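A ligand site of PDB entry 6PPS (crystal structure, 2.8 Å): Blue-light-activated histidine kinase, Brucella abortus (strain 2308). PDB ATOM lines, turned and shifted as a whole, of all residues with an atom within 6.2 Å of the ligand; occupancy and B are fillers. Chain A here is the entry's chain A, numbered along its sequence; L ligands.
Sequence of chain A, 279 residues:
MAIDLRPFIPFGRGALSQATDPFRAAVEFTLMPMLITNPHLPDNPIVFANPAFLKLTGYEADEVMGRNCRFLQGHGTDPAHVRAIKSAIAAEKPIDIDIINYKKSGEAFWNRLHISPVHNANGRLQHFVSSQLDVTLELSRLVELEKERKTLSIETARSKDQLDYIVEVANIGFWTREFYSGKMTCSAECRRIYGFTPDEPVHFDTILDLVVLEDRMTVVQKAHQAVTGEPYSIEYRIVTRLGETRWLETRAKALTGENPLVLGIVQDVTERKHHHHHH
The side-chain amide oxygen (OD1) of Asn 68 sits at hydrogen-bond distance from the backbone NH (N) of Arg 70, at 2.9 Å.
NH1 of Arg 70 is in salt-bridge range of OD1 of Asp 43, at 2.9 Å.
The backbone carbonyl oxygen (O) of Asn 44 lies within hydrogen-bond range of the side-chain amide nitrogen (ND2) of Asn 68.
The backbone carbonyl oxygen of Asp 43 is in hydrogen-bond range of the side-chain amide nitrogen of Asn 68 (2.5 Å).
ND2 of Asn 101 sits close to O of Leu 72, 3.5 Å away.
The side-chain amide oxygen (OD1) of Asn 101 sits at hydrogen-bond distance from the side-chain amide nitrogen (ND2) of Asn 111.
The backbone NH (N) of Ser 130 lies within hydrogen-bond range of the backbone carbonyl oxygen (O) of Leu 35, 2.9 Å away.
N of Thr 37 lies within hydrogen-bond range of O of Phe 128 (2.9 Å).
The side-chain amide nitrogen (NE2) of Gln 73 is in hydrogen-bond range of an oxygen (O5) of the ligand, 2.5 Å away.
The guanidinium group of Arg 70 is in salt-bridge range of an oxygen (O8) of the ligand (2.6 Å).
The side-chain amide oxygen of Asn 68 lies within hydrogen-bond range of an oxygen (O3) of the ligand, at 2.7 Å.
The side-chain amide nitrogen (ND2) of Asn 101 lies within hydrogen-bond range of an oxygen (O1) of the ligand (2.7 Å).
The side-chain amide nitrogen (NE2) of Gln 132 sits at hydrogen-bond distance from an oxygen (O2) of the ligand, 2.9 Å away.
The backbone NH of Cys 69 lies close to an oxygen (O3) of the ligand, at 3.5 Å.
NZ of Lys 86 lies within salt-bridge range of O7 of the ligand, at 3.6 Å.
ND2 of Asn 111 sits at hydrogen-bond distance from O2 of the ligand, 3.5 Å away.
Thr 37 touches the ligand.
Asn 44 touches the ligand (ND2 to C9, 3.6 Å).
Leu 72 touches the ligand (CD1 to O2, 3.4 Å).
Val 82 touches the ligand.
CG2 of Ile 85 touches C13 of the ligand, 3.6 Å away.
Ile 89 touches the ligand.
Ile 99 touches the ligand.
Leu 113 touches the ligand (CD1 to O2, 3.4 Å).
Ile 115 touches the ligand.
Phe 128 touches the ligand (CB to C9, 3.8 Å).
Ser 130 touches the ligand (OG to C5, 3.4 Å).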
ATOM      1  N   LEU A  35      16.628  -9.364  -2.574  1.00  0.00           N
ATOM      2  CA  LEU A  35      15.447 -10.017  -3.145  1.00  0.00           C
ATOM      3  C   LEU A  35      14.830 -11.018  -2.185  1.00  0.00           C
ATOM      4  O   LEU A  35      15.533 -11.635  -1.373  1.00  0.00           O
ATOM      5  CB  LEU A  35      15.807 -10.717  -4.456  1.00  0.00           C
ATOM      6  CG  LEU A  35      16.159  -9.870  -5.668  1.00  0.00           C
ATOM      7  CD1 LEU A  35      16.372 -10.760  -6.873  1.00  0.00           C
ATOM      8  CD2 LEU A  35      15.078  -8.844  -5.945  1.00  0.00           C
ATOM      9  N   ILE A  36      13.514 -11.178  -2.282  1.00  0.00           N
ATOM     10  CA  ILE A  36      12.802 -12.205  -1.530  1.00  0.00           C
ATOM     11  C   ILE A  36      11.849 -12.963  -2.457  1.00  0.00           C
ATOM     12  O   ILE A  36      11.054 -12.349  -3.167  1.00  0.00           O
ATOM     13  CB  ILE A  36      11.999 -11.603  -0.358  1.00  0.00           C
ATOM     14  CG1 ILE A  36      12.923 -10.866   0.616  1.00  0.00           C
ATOM     15  CG2 ILE A  36      11.235 -12.703   0.371  1.00  0.00           C
ATOM     16  CD1 ILE A  36      12.199 -10.240   1.777  1.00  0.00           C
ATOM     17  N   THR A  37      11.955 -14.290  -2.459  1.00  0.00           N
ATOM     18  CA  THR A  37      11.076 -15.104  -3.294  1.00  0.00           C
ATOM     19  C   THR A  37      10.233 -16.051  -2.459  1.00  0.00           C
ATOM     20  O   THR A  37      10.609 -16.426  -1.345  1.00  0.00           O
ATOM     21  CB  THR A  37      11.887 -15.922  -4.320  1.00  0.00           C
ATOM     22  OG1 THR A  37      12.654 -16.927  -3.640  1.00  0.00           O
ATOM     23  CG2 THR A  37      12.813 -15.026  -5.120  1.00  0.00           C
ATOM     24  N   ASP A  43       7.469 -21.929  -9.893  1.00  0.00           N
ATOM     25  CA  ASP A  43       8.661 -21.315 -10.492  1.00  0.00           C
ATOM     26  C   ASP A  43       9.420 -20.394  -9.524  1.00  0.00           C
ATOM     27  O   ASP A  43      10.388 -19.742  -9.919  1.00  0.00           O
ATOM     28  CB  ASP A  43       8.288 -20.548 -11.761  1.00  0.00           C
ATOM     29  CG  ASP A  43       9.481 -20.306 -12.670  1.00  0.00           C
ATOM     30  OD1 ASP A  43      10.460 -21.086 -12.593  1.00  0.00           O
ATOM     31  OD2 ASP A  43       9.449 -19.350 -13.459  1.00  0.00           O
ATOM     32  N   ASN A  44       8.984 -20.352  -8.265  1.00  0.00           N
ATOM     33  CA  ASN A  44       9.645 -19.573  -7.222  1.00  0.00           C
ATOM     34  C   ASN A  44       9.884 -18.114  -7.631  1.00  0.00           C
ATOM     35  O   ASN A  44      11.024 -17.714  -7.879  1.00  0.00           O
ATOM     36  CB  ASN A  44      10.977 -20.232  -6.851  1.00  0.00           C
ATOM     37  CG  ASN A  44      11.620 -19.614  -5.623  1.00  0.00           C
ATOM     38  OD1 ASN A  44      10.939 -19.023  -4.784  1.00  0.00           O
ATOM     39  ND2 ASN A  44      12.931 -19.736  -5.519  1.00  0.00           N
ATOM     40  N   PHE A  53      17.856  -2.656  -5.651  1.00  0.00           N
ATOM     41  CA  PHE A  53      17.794  -3.663  -6.713  1.00  0.00           C
ATOM     42  C   PHE A  53      17.194  -3.076  -7.993  1.00  0.00           C
ATOM     43  O   PHE A  53      17.726  -3.294  -9.084  1.00  0.00           O
ATOM     44  CB  PHE A  53      16.973  -4.874  -6.258  1.00  0.00           C
ATOM     45  CG  PHE A  53      16.784  -5.915  -7.321  1.00  0.00           C
ATOM     46  CD1 PHE A  53      15.648  -5.917  -8.122  1.00  0.00           C
ATOM     47  CD2 PHE A  53      17.745  -6.892  -7.529  1.00  0.00           C
ATOM     48  CE1 PHE A  53      15.467  -6.872  -9.097  1.00  0.00           C
ATOM     49  CE2 PHE A  53      17.572  -7.851  -8.514  1.00  0.00           C
ATOM     50  CZ  PHE A  53      16.432  -7.845  -9.292  1.00  0.00           C
ATOM     51  N   ASN A  68      10.521 -15.310 -12.057  1.00  0.00           N
ATOM     52  CA  ASN A  68      11.731 -15.919 -11.505  1.00  0.00           C
ATOM     53  C   ASN A  68      12.940 -15.034 -11.786  1.00  0.00           C
ATOM     54  O   ASN A  68      12.935 -14.262 -12.748  1.00  0.00           O
ATOM     55  CB  ASN A  68      11.946 -17.313 -12.097  1.00  0.00           C
ATOM     56  CG  ASN A  68      13.072 -18.065 -11.412  1.00  0.00           C
ATOM     57  OD1 ASN A  68      14.244 -17.870 -11.711  1.00  0.00           O
ATOM     58  ND2 ASN A  68      12.713 -18.939 -10.469  1.00  0.00           N
ATOM     59  N   CYS A  69      13.970 -15.152 -10.961  1.00  0.00           N
ATOM     60  CA  CYS A  69      15.144 -14.295 -11.060  1.00  0.00           C
ATOM     61  C   CYS A  69      16.040 -14.639 -12.246  1.00  0.00           C
ATOM     62  O   CYS A  69      17.064 -13.990 -12.465  1.00  0.00           O
ATOM     63  CB  CYS A  69      15.963 -14.378  -9.770  1.00  0.00           C
ATOM     64  SG  CYS A  69      14.996 -14.222  -8.257  1.00  0.00           S
ATOM     65  N   ARG A  70      15.655 -15.646 -13.020  1.00  0.00           N
ATOM     66  CA  ARG A  70      16.476 -16.085 -14.145  1.00  0.00           C
ATOM     67  C   ARG A  70      16.383 -15.126 -15.326  1.00  0.00           C
ATOM     68  O   ARG A  70      17.107 -15.275 -16.317  1.00  0.00           O
ATOM     69  CB  ARG A  70      16.084 -17.499 -14.581  1.00  0.00           C
ATOM     70  CG  ARG A  70      14.758 -17.569 -15.321  1.00  0.00           C
ATOM     71  CD  ARG A  70      14.524 -18.962 -15.878  1.00  0.00           C
ATOM     72  NE  ARG A  70      14.498 -19.969 -14.822  1.00  0.00           N
ATOM     73  CZ  ARG A  70      13.402 -20.336 -14.165  1.00  0.00           C
ATOM     74  NH1 ARG A  70      12.237 -19.770 -14.449  1.00  0.00           N
ATOM     75  NH2 ARG A  70      13.470 -21.262 -13.218  1.00  0.00           N
ATOM     76  N   LEU A  72      17.338 -12.189 -15.373  1.00  0.00           N
ATOM     77  CA  LEU A  72      18.528 -11.341 -15.366  1.00  0.00           C
ATOM     78  C   LEU A  72      19.661 -11.954 -16.173  1.00  0.00           C
ATOM     79  O   LEU A  72      20.656 -11.291 -16.472  1.00  0.00           O
ATOM     80  CB  LEU A  72      18.987 -11.086 -13.923  1.00  0.00           C
ATOM     81  CG  LEU A  72      18.123 -10.166 -13.057  1.00  0.00           C
ATOM     82  CD1 LEU A  72      18.718 -10.075 -11.657  1.00  0.00           C
ATOM     83  CD2 LEU A  72      18.007  -8.794 -13.684  1.00  0.00           C
ATOM     84  N   GLN A  73      19.505 -13.230 -16.536  1.00  0.00           N
ATOM     85  CA  GLN A  73      20.557 -13.965 -17.241  1.00  0.00           C
ATOM     86  C   GLN A  73      20.542 -13.681 -18.738  1.00  0.00           C
ATOM     87  O   GLN A  73      19.537 -13.246 -19.292  1.00  0.00           O
ATOM     88  CB  GLN A  73      20.405 -15.462 -16.982  1.00  0.00           C
ATOM     89  CG  GLN A  73      20.531 -15.844 -15.525  1.00  0.00           C
ATOM     90  CD  GLN A  73      20.154 -17.282 -15.254  1.00  0.00           C
ATOM     91  OE1 GLN A  73      19.724 -18.008 -16.150  1.00  0.00           O
ATOM     92  NE2 GLN A  73      20.307 -17.705 -14.004  1.00  0.00           N
ATOM     93  N   THR A  77      26.099 -15.428 -19.483  1.00  0.00           N
ATOM     94  CA  THR A  77      25.834 -16.189 -18.263  1.00  0.00           C
ATOM     95  C   THR A  77      26.373 -17.606 -18.385  1.00  0.00           C
ATOM     96  O   THR A  77      25.917 -18.382 -19.227  1.00  0.00           O
ATOM     97  CB  THR A  77      24.334 -16.231 -17.945  1.00  0.00           C
ATOM     98  OG1 THR A  77      23.829 -14.899 -17.817  1.00  0.00           O
ATOM     99  CG2 THR A  77      24.078 -16.984 -16.645  1.00  0.00           C
ATOM    100  N   VAL A  82      24.674 -21.595 -13.446  1.00  0.00           N
ATOM    101  CA  VAL A  82      23.236 -21.754 -13.323  1.00  0.00           C
ATOM    102  C   VAL A  82      22.879 -23.102 -12.697  1.00  0.00           C
ATOM    103  O   VAL A  82      21.957 -23.190 -11.880  1.00  0.00           O
ATOM    104  CB  VAL A  82      22.537 -21.630 -14.696  1.00  0.00           C
ATOM    105  CG1 VAL A  82      21.020 -21.766 -14.546  1.00  0.00           C
ATOM    106  CG2 VAL A  82      22.877 -20.302 -15.349  1.00  0.00           C
ATOM    107  N   ARG A  83      23.618 -24.146 -13.067  1.00  0.00           N
ATOM    108  CA  ARG A  83      23.374 -25.472 -12.532  1.00  0.00           C
ATOM    109  C   ARG A  83      23.657 -25.544 -11.034  1.00  0.00           C
ATOM    110  O   ARG A  83      22.951 -26.235 -10.298  1.00  0.00           O
ATOM    111  CB  ARG A  83      24.234 -26.522 -13.258  1.00  0.00           C
ATOM    112  CG  ARG A  83      23.799 -26.796 -14.689  1.00  0.00           C
ATOM    113  CD  ARG A  83      24.386 -28.114 -15.189  1.00  0.00           C
ATOM    114  NE  ARG A  83      25.833 -28.150 -15.071  1.00  0.00           N
ATOM    115  CZ  ARG A  83      26.672 -27.777 -16.038  1.00  0.00           C
ATOM    116  NH1 ARG A  83      26.195 -27.335 -17.192  1.00  0.00           N
ATOM    117  NH2 ARG A  83      27.980 -27.848 -15.847  1.00  0.00           N
ATOM    118  N   ILE A  85      23.360 -23.087  -8.827  1.00  0.00           N
ATOM    119  CA  ILE A  85      22.260 -22.421  -8.132  1.00  0.00           C
ATOM    120  C   ILE A  85      21.031 -23.327  -8.094  1.00  0.00           C
ATOM    121  O   ILE A  85      20.362 -23.428  -7.063  1.00  0.00           O
ATOM    122  CB  ILE A  85      21.891 -21.092  -8.816  1.00  0.00           C
ATOM    123  CG1 ILE A  85      23.128 -20.196  -8.948  1.00  0.00           C
ATOM    124  CG2 ILE A  85      20.802 -20.377  -8.031  1.00  0.00           C
ATOM    125  CD1 ILE A  85      22.843 -18.855  -9.587  1.00  0.00           C
ATOM    126  N   LYS A  86      20.748 -23.974  -9.218  1.00  0.00           N
ATOM    127  CA  LYS A  86      19.601 -24.872  -9.325  1.00  0.00           C
ATOM    128  C   LYS A  86      19.685 -26.016  -8.320  1.00  0.00           C
ATOM    129  O   LYS A  86      18.706 -26.329  -7.641  1.00  0.00           O
ATOM    130  CB  LYS A  86      19.480 -25.434 -10.739  1.00  0.00           C
ATOM    131  CG  LYS A  86      18.410 -26.491 -10.887  1.00  0.00           C
ATOM    132  CD  LYS A  86      18.355 -27.038 -12.296  1.00  0.00           C
ATOM    133  CE  LYS A  86      17.278 -28.111 -12.422  1.00  0.00           C
ATOM    134  NZ  LYS A  86      15.938 -27.581 -12.040  1.00  0.00           N
ATOM    135  N   ILE A  89      19.161 -24.663  -4.682  1.00  0.00           N
ATOM    136  CA  ILE A  89      17.778 -24.310  -4.419  1.00  0.00           C
ATOM    137  C   ILE A  89      16.905 -25.560  -4.291  1.00  0.00           C
ATOM    138  O   ILE A  89      16.042 -25.644  -3.416  1.00  0.00           O
ATOM    139  CB  ILE A  89      17.214 -23.392  -5.521  1.00  0.00           C
ATOM    140  CG1 ILE A  89      17.942 -22.054  -5.509  1.00  0.00           C
ATOM    141  CG2 ILE A  89      15.715 -23.173  -5.342  1.00  0.00           C
ATOM    142  CD1 ILE A  89      17.510 -21.108  -6.602  1.00  0.00           C
ATOM    143  N   ILE A  99      27.910 -14.606 -10.683  1.00  0.00           N
ATOM    144  CA  ILE A  99      27.315 -14.917 -11.986  1.00  0.00           C
ATOM    145  C   ILE A  99      27.199 -13.646 -12.824  1.00  0.00           C
ATOM    146  O   ILE A  99      27.197 -12.534 -12.306  1.00  0.00           O
ATOM    147  CB  ILE A  99      25.931 -15.578 -11.828  1.00  0.00           C
ATOM    148  CG1 ILE A  99      25.577 -16.411 -13.059  1.00  0.00           C
ATOM    149  CG2 ILE A  99      24.867 -14.532 -11.535  1.00  0.00           C
ATOM    150  CD1 ILE A  99      24.278 -17.162 -12.918  1.00  0.00           C
ATOM    151  N   ILE A 100      27.112 -13.820 -14.146  1.00  0.00           N
ATOM    152  CA  ILE A 100      26.950 -12.689 -15.051  1.00  0.00           C
ATOM    153  C   ILE A 100      25.471 -12.425 -15.334  1.00  0.00           C
ATOM    154  O   ILE A 100      24.778 -13.267 -15.906  1.00  0.00           O
ATOM    155  CB  ILE A 100      27.681 -12.932 -16.390  1.00  0.00           C
ATOM    156  CG1 ILE A 100      29.191 -12.948 -16.167  1.00  0.00           C
ATOM    157  CG2 ILE A 100      27.307 -11.855 -17.401  1.00  0.00           C
ATOM    158  CD1 ILE A 100      29.999 -13.124 -17.434  1.00  0.00           C
ATOM    159  N   ASN A 101      24.995 -11.258 -14.919  1.00  0.00           N
ATOM    160  CA  ASN A 101      23.625 -10.857 -15.178  1.00  0.00           C
ATOM    161  C   ASN A 101      23.545  -9.652 -16.095  1.00  0.00           C
ATOM    162  O   ASN A 101      24.580  -9.104 -16.505  1.00  0.00           O
ATOM    163  CB  ASN A 101      22.889 -10.573 -13.866  1.00  0.00           C
ATOM    164  CG  ASN A 101      22.581 -11.838 -13.088  1.00  0.00           C
ATOM    165  OD1 ASN A 101      22.644 -11.859 -11.856  1.00  0.00           O
ATOM    166  ND2 ASN A 101      22.234 -12.906 -13.804  1.00  0.00           N
ATOM    167  N   ASN A 111      27.312 -10.065 -10.901  1.00  0.00           N
ATOM    168  CA  ASN A 111      26.427 -10.096  -9.748  1.00  0.00           C
ATOM    169  C   ASN A 111      26.894 -11.095  -8.698  1.00  0.00           C
ATOM    170  O   ASN A 111      26.762 -12.302  -8.872  1.00  0.00           O
ATOM    171  CB  ASN A 111      24.999 -10.434 -10.189  1.00  0.00           C
ATOM    172  CG  ASN A 111      23.959 -10.147  -9.115  1.00  0.00           C
ATOM    173  OD1 ASN A 111      24.261 -10.146  -7.924  1.00  0.00           O
ATOM    174  ND2 ASN A 111      22.726  -9.904  -9.537  1.00  0.00           N
ATOM    175  N   LEU A 113      26.227 -13.135  -5.912  1.00  0.00           N
ATOM    176  CA  LEU A 113      24.987 -13.666  -5.352  1.00  0.00           C
ATOM    177  C   LEU A 113      25.186 -14.334  -3.999  1.00  0.00           C
ATOM    178  O   LEU A 113      26.028 -15.220  -3.853  1.00  0.00           O
ATOM    179  CB  LEU A 113      24.369 -14.666  -6.329  1.00  0.00           C
ATOM    180  CG  LEU A 113      22.950 -14.406  -6.817  1.00  0.00           C
ATOM    181  CD1 LEU A 113      22.858 -13.087  -7.561  1.00  0.00           C
ATOM    182  CD2 LEU A 113      22.477 -15.554  -7.699  1.00  0.00           C
ATOM    183  N   ILE A 115      22.636 -16.283  -1.611  1.00  0.00           N
ATOM    184  CA  ILE A 115      21.279 -16.786  -1.415  1.00  0.00           C
ATOM    185  C   ILE A 115      21.166 -17.630  -0.159  1.00  0.00           C
ATOM    186  O   ILE A 115      22.015 -18.487   0.107  1.00  0.00           O
ATOM    187  CB  ILE A 115      20.821 -17.610  -2.637  1.00  0.00           C
ATOM    188  CG1 ILE A 115      20.968 -16.793  -3.919  1.00  0.00           C
ATOM    189  CG2 ILE A 115      19.390 -18.085  -2.455  1.00  0.00           C
ATOM    190  CD1 ILE A 115      20.562 -17.544  -5.172  1.00  0.00           C
ATOM    191  N   SER A 116      20.115 -17.391   0.621  1.00  0.00           N
ATOM    192  CA  SER A 116      19.862 -18.144   1.850  1.00  0.00           C
ATOM    193  C   SER A 116      18.414 -18.595   1.938  1.00  0.00           C
ATOM    194  O   SER A 116      17.494 -17.801   1.721  1.00  0.00           O
ATOM    195  CB  SER A 116      20.226 -17.316   3.072  1.00  0.00           C
ATOM    196  OG  SER A 116      21.592 -16.931   3.055  1.00  0.00           O
ATOM    197  N   PHE A 128      12.971 -17.704   0.332  1.00  0.00           N
ATOM    198  CA  PHE A 128      14.363 -17.530  -0.089  1.00  0.00           C
ATOM    199  C   PHE A 128      14.700 -16.045  -0.074  1.00  0.00           C
ATOM    200  O   PHE A 128      13.939 -15.223  -0.585  1.00  0.00           O
ATOM    201  CB  PHE A 128      14.584 -18.104  -1.498  1.00  0.00           C
ATOM    202  CG  PHE A 128      14.799 -19.588  -1.522  1.00  0.00           C
ATOM    203  CD1 PHE A 128      15.988 -20.142  -1.072  1.00  0.00           C
ATOM    204  CD2 PHE A 128      13.816 -20.439  -2.025  1.00  0.00           C
ATOM    205  CE1 PHE A 128      16.188 -21.510  -1.109  1.00  0.00           C
ATOM    206  CE2 PHE A 128      14.011 -21.802  -2.069  1.00  0.00           C
ATOM    207  CZ  PHE A 128      15.199 -22.340  -1.608  1.00  0.00           C
ATOM    208  N   VAL A 129      15.833 -15.699   0.518  1.00  0.00           N
ATOM    209  CA  VAL A 129      16.293 -14.323   0.532  1.00  0.00           C
ATOM    210  C   VAL A 129      17.701 -14.214  -0.062  1.00  0.00           C
ATOM    211  O   VAL A 129      18.501 -15.145   0.057  1.00  0.00           O
ATOM    212  CB  VAL A 129      16.290 -13.729   1.954  1.00  0.00           C
ATOM    213  CG1 VAL A 129      14.860 -13.477   2.418  1.00  0.00           C
ATOM    214  CG2 VAL A 129      17.019 -14.655   2.925  1.00  0.00           C
ATOM    215  N   SER A 130      17.998 -13.098  -0.707  1.00  0.00           N
ATOM    216  CA  SER A 130      19.284 -12.937  -1.375  1.00  0.00           C
ATOM    217  C   SER A 130      19.841 -11.529  -1.273  1.00  0.00           C
ATOM    218  O   SER A 130      19.101 -10.541  -1.236  1.00  0.00           O
ATOM    219  CB  SER A 130      19.150 -13.326  -2.851  1.00  0.00           C
ATOM    220  OG  SER A 130      18.362 -12.388  -3.558  1.00  0.00           O
ATOM    221  N   GLN A 132      22.194  -9.248  -3.406  1.00  0.00           N
ATOM    222  CA  GLN A 132      22.923  -8.994  -4.641  1.00  0.00           C
ATOM    223  C   GLN A 132      23.929  -7.869  -4.475  1.00  0.00           C
ATOM    224  O   GLN A 132      23.652  -6.866  -3.809  1.00  0.00           O
ATOM    225  CB  GLN A 132      21.940  -8.657  -5.771  1.00  0.00           C
ATOM    226  CG  GLN A 132      21.364  -9.876  -6.505  1.00  0.00           C
ATOM    227  CD  GLN A 132      20.333 -10.638  -5.699  1.00  0.00           C
ATOM    228  OE1 GLN A 132      20.157 -10.411  -4.506  1.00  0.00           O
ATOM    229  NE2 GLN A 132      19.631 -11.545  -6.373  1.00  0.00           N
HETATM  230  N1  LIG L   1      19.891 -15.787 -10.785  1.00  0.00           N
HETATM  231  C1  LIG L   1      20.529 -14.774 -11.454  1.00  0.00           C
HETATM  232  O1  LIG L   1      21.061 -14.992 -12.546  1.00  0.00           O
HETATM  233  N2  LIG L   1      20.589 -13.500 -10.919  1.00  0.00           N
HETATM  234  C2  LIG L   1      19.998 -13.242  -9.694  1.00  0.00           C
HETATM  235  O2  LIG L   1      20.052 -12.112  -9.216  1.00  0.00           O
HETATM  236  C3  LIG L   1      19.356 -14.263  -9.014  1.00  0.00           C
HETATM  237  N3  LIG L   1      18.765 -14.006  -7.790  1.00  0.00           N
HETATM  238  C4  LIG L   1      18.132 -15.015  -7.108  1.00  0.00           C
HETATM  239  C5  LIG L   1      17.540 -14.749  -5.878  1.00  0.00           C
HETATM  240  C6  LIG L   1      16.889 -15.765  -5.189  1.00  0.00           C
HETATM  241  C7  LIG L   1      16.252 -15.482  -3.864  1.00  0.00           C
HETATM  242  C8  LIG L   1      16.829 -17.047  -5.730  1.00  0.00           C
HETATM  243  C9  LIG L   1      16.129 -18.149  -4.991  1.00  0.00           C
HETATM  244  C10 LIG L   1      17.421 -17.313  -6.960  1.00  0.00           C
HETATM  245  C11 LIG L   1      18.067 -16.293  -7.656  1.00  0.00           C
HETATM  246  N4  LIG L   1      18.650 -16.554  -8.877  1.00  0.00           N
HETATM  247  C12 LIG L   1      19.297 -15.545  -9.555  1.00  0.00           C
HETATM  248  C13 LIG L   1      18.599 -17.940  -9.460  1.00  0.00           C
HETATM  249  C14 LIG L   1      17.480 -18.069 -10.484  1.00  0.00           C
HETATM  250  O3  LIG L   1      16.273 -17.582  -9.948  1.00  0.00           O
HETATM  251  C15 LIG L   1      17.304 -19.523 -10.888  1.00  0.00           C
HETATM  252  O4  LIG L   1      17.029 -20.300  -9.753  1.00  0.00           O
HETATM  253  C16 LIG L   1      18.562 -20.057 -11.583  1.00  0.00           C
HETATM  254  O5  LIG L   1      18.857 -19.261 -12.707  1.00  0.00           O
HETATM  255  C17 LIG L   1      18.366 -21.502 -12.022  1.00  0.00           C
HETATM  256  O6  LIG L   1      17.142 -21.597 -12.711  1.00  0.00           O
HETATM  257  P1  LIG L   1      16.794 -22.921 -13.568  1.00  0.00           P
HETATM  258  O7  LIG L   1      16.890 -24.120 -12.659  1.00  0.00           O
HETATM  259  O8  LIG L   1      15.387 -22.810 -14.101  1.00  0.00           O
HETATM  260  O9  LIG L   1      17.765 -23.054 -14.717  1.00  0.00           O
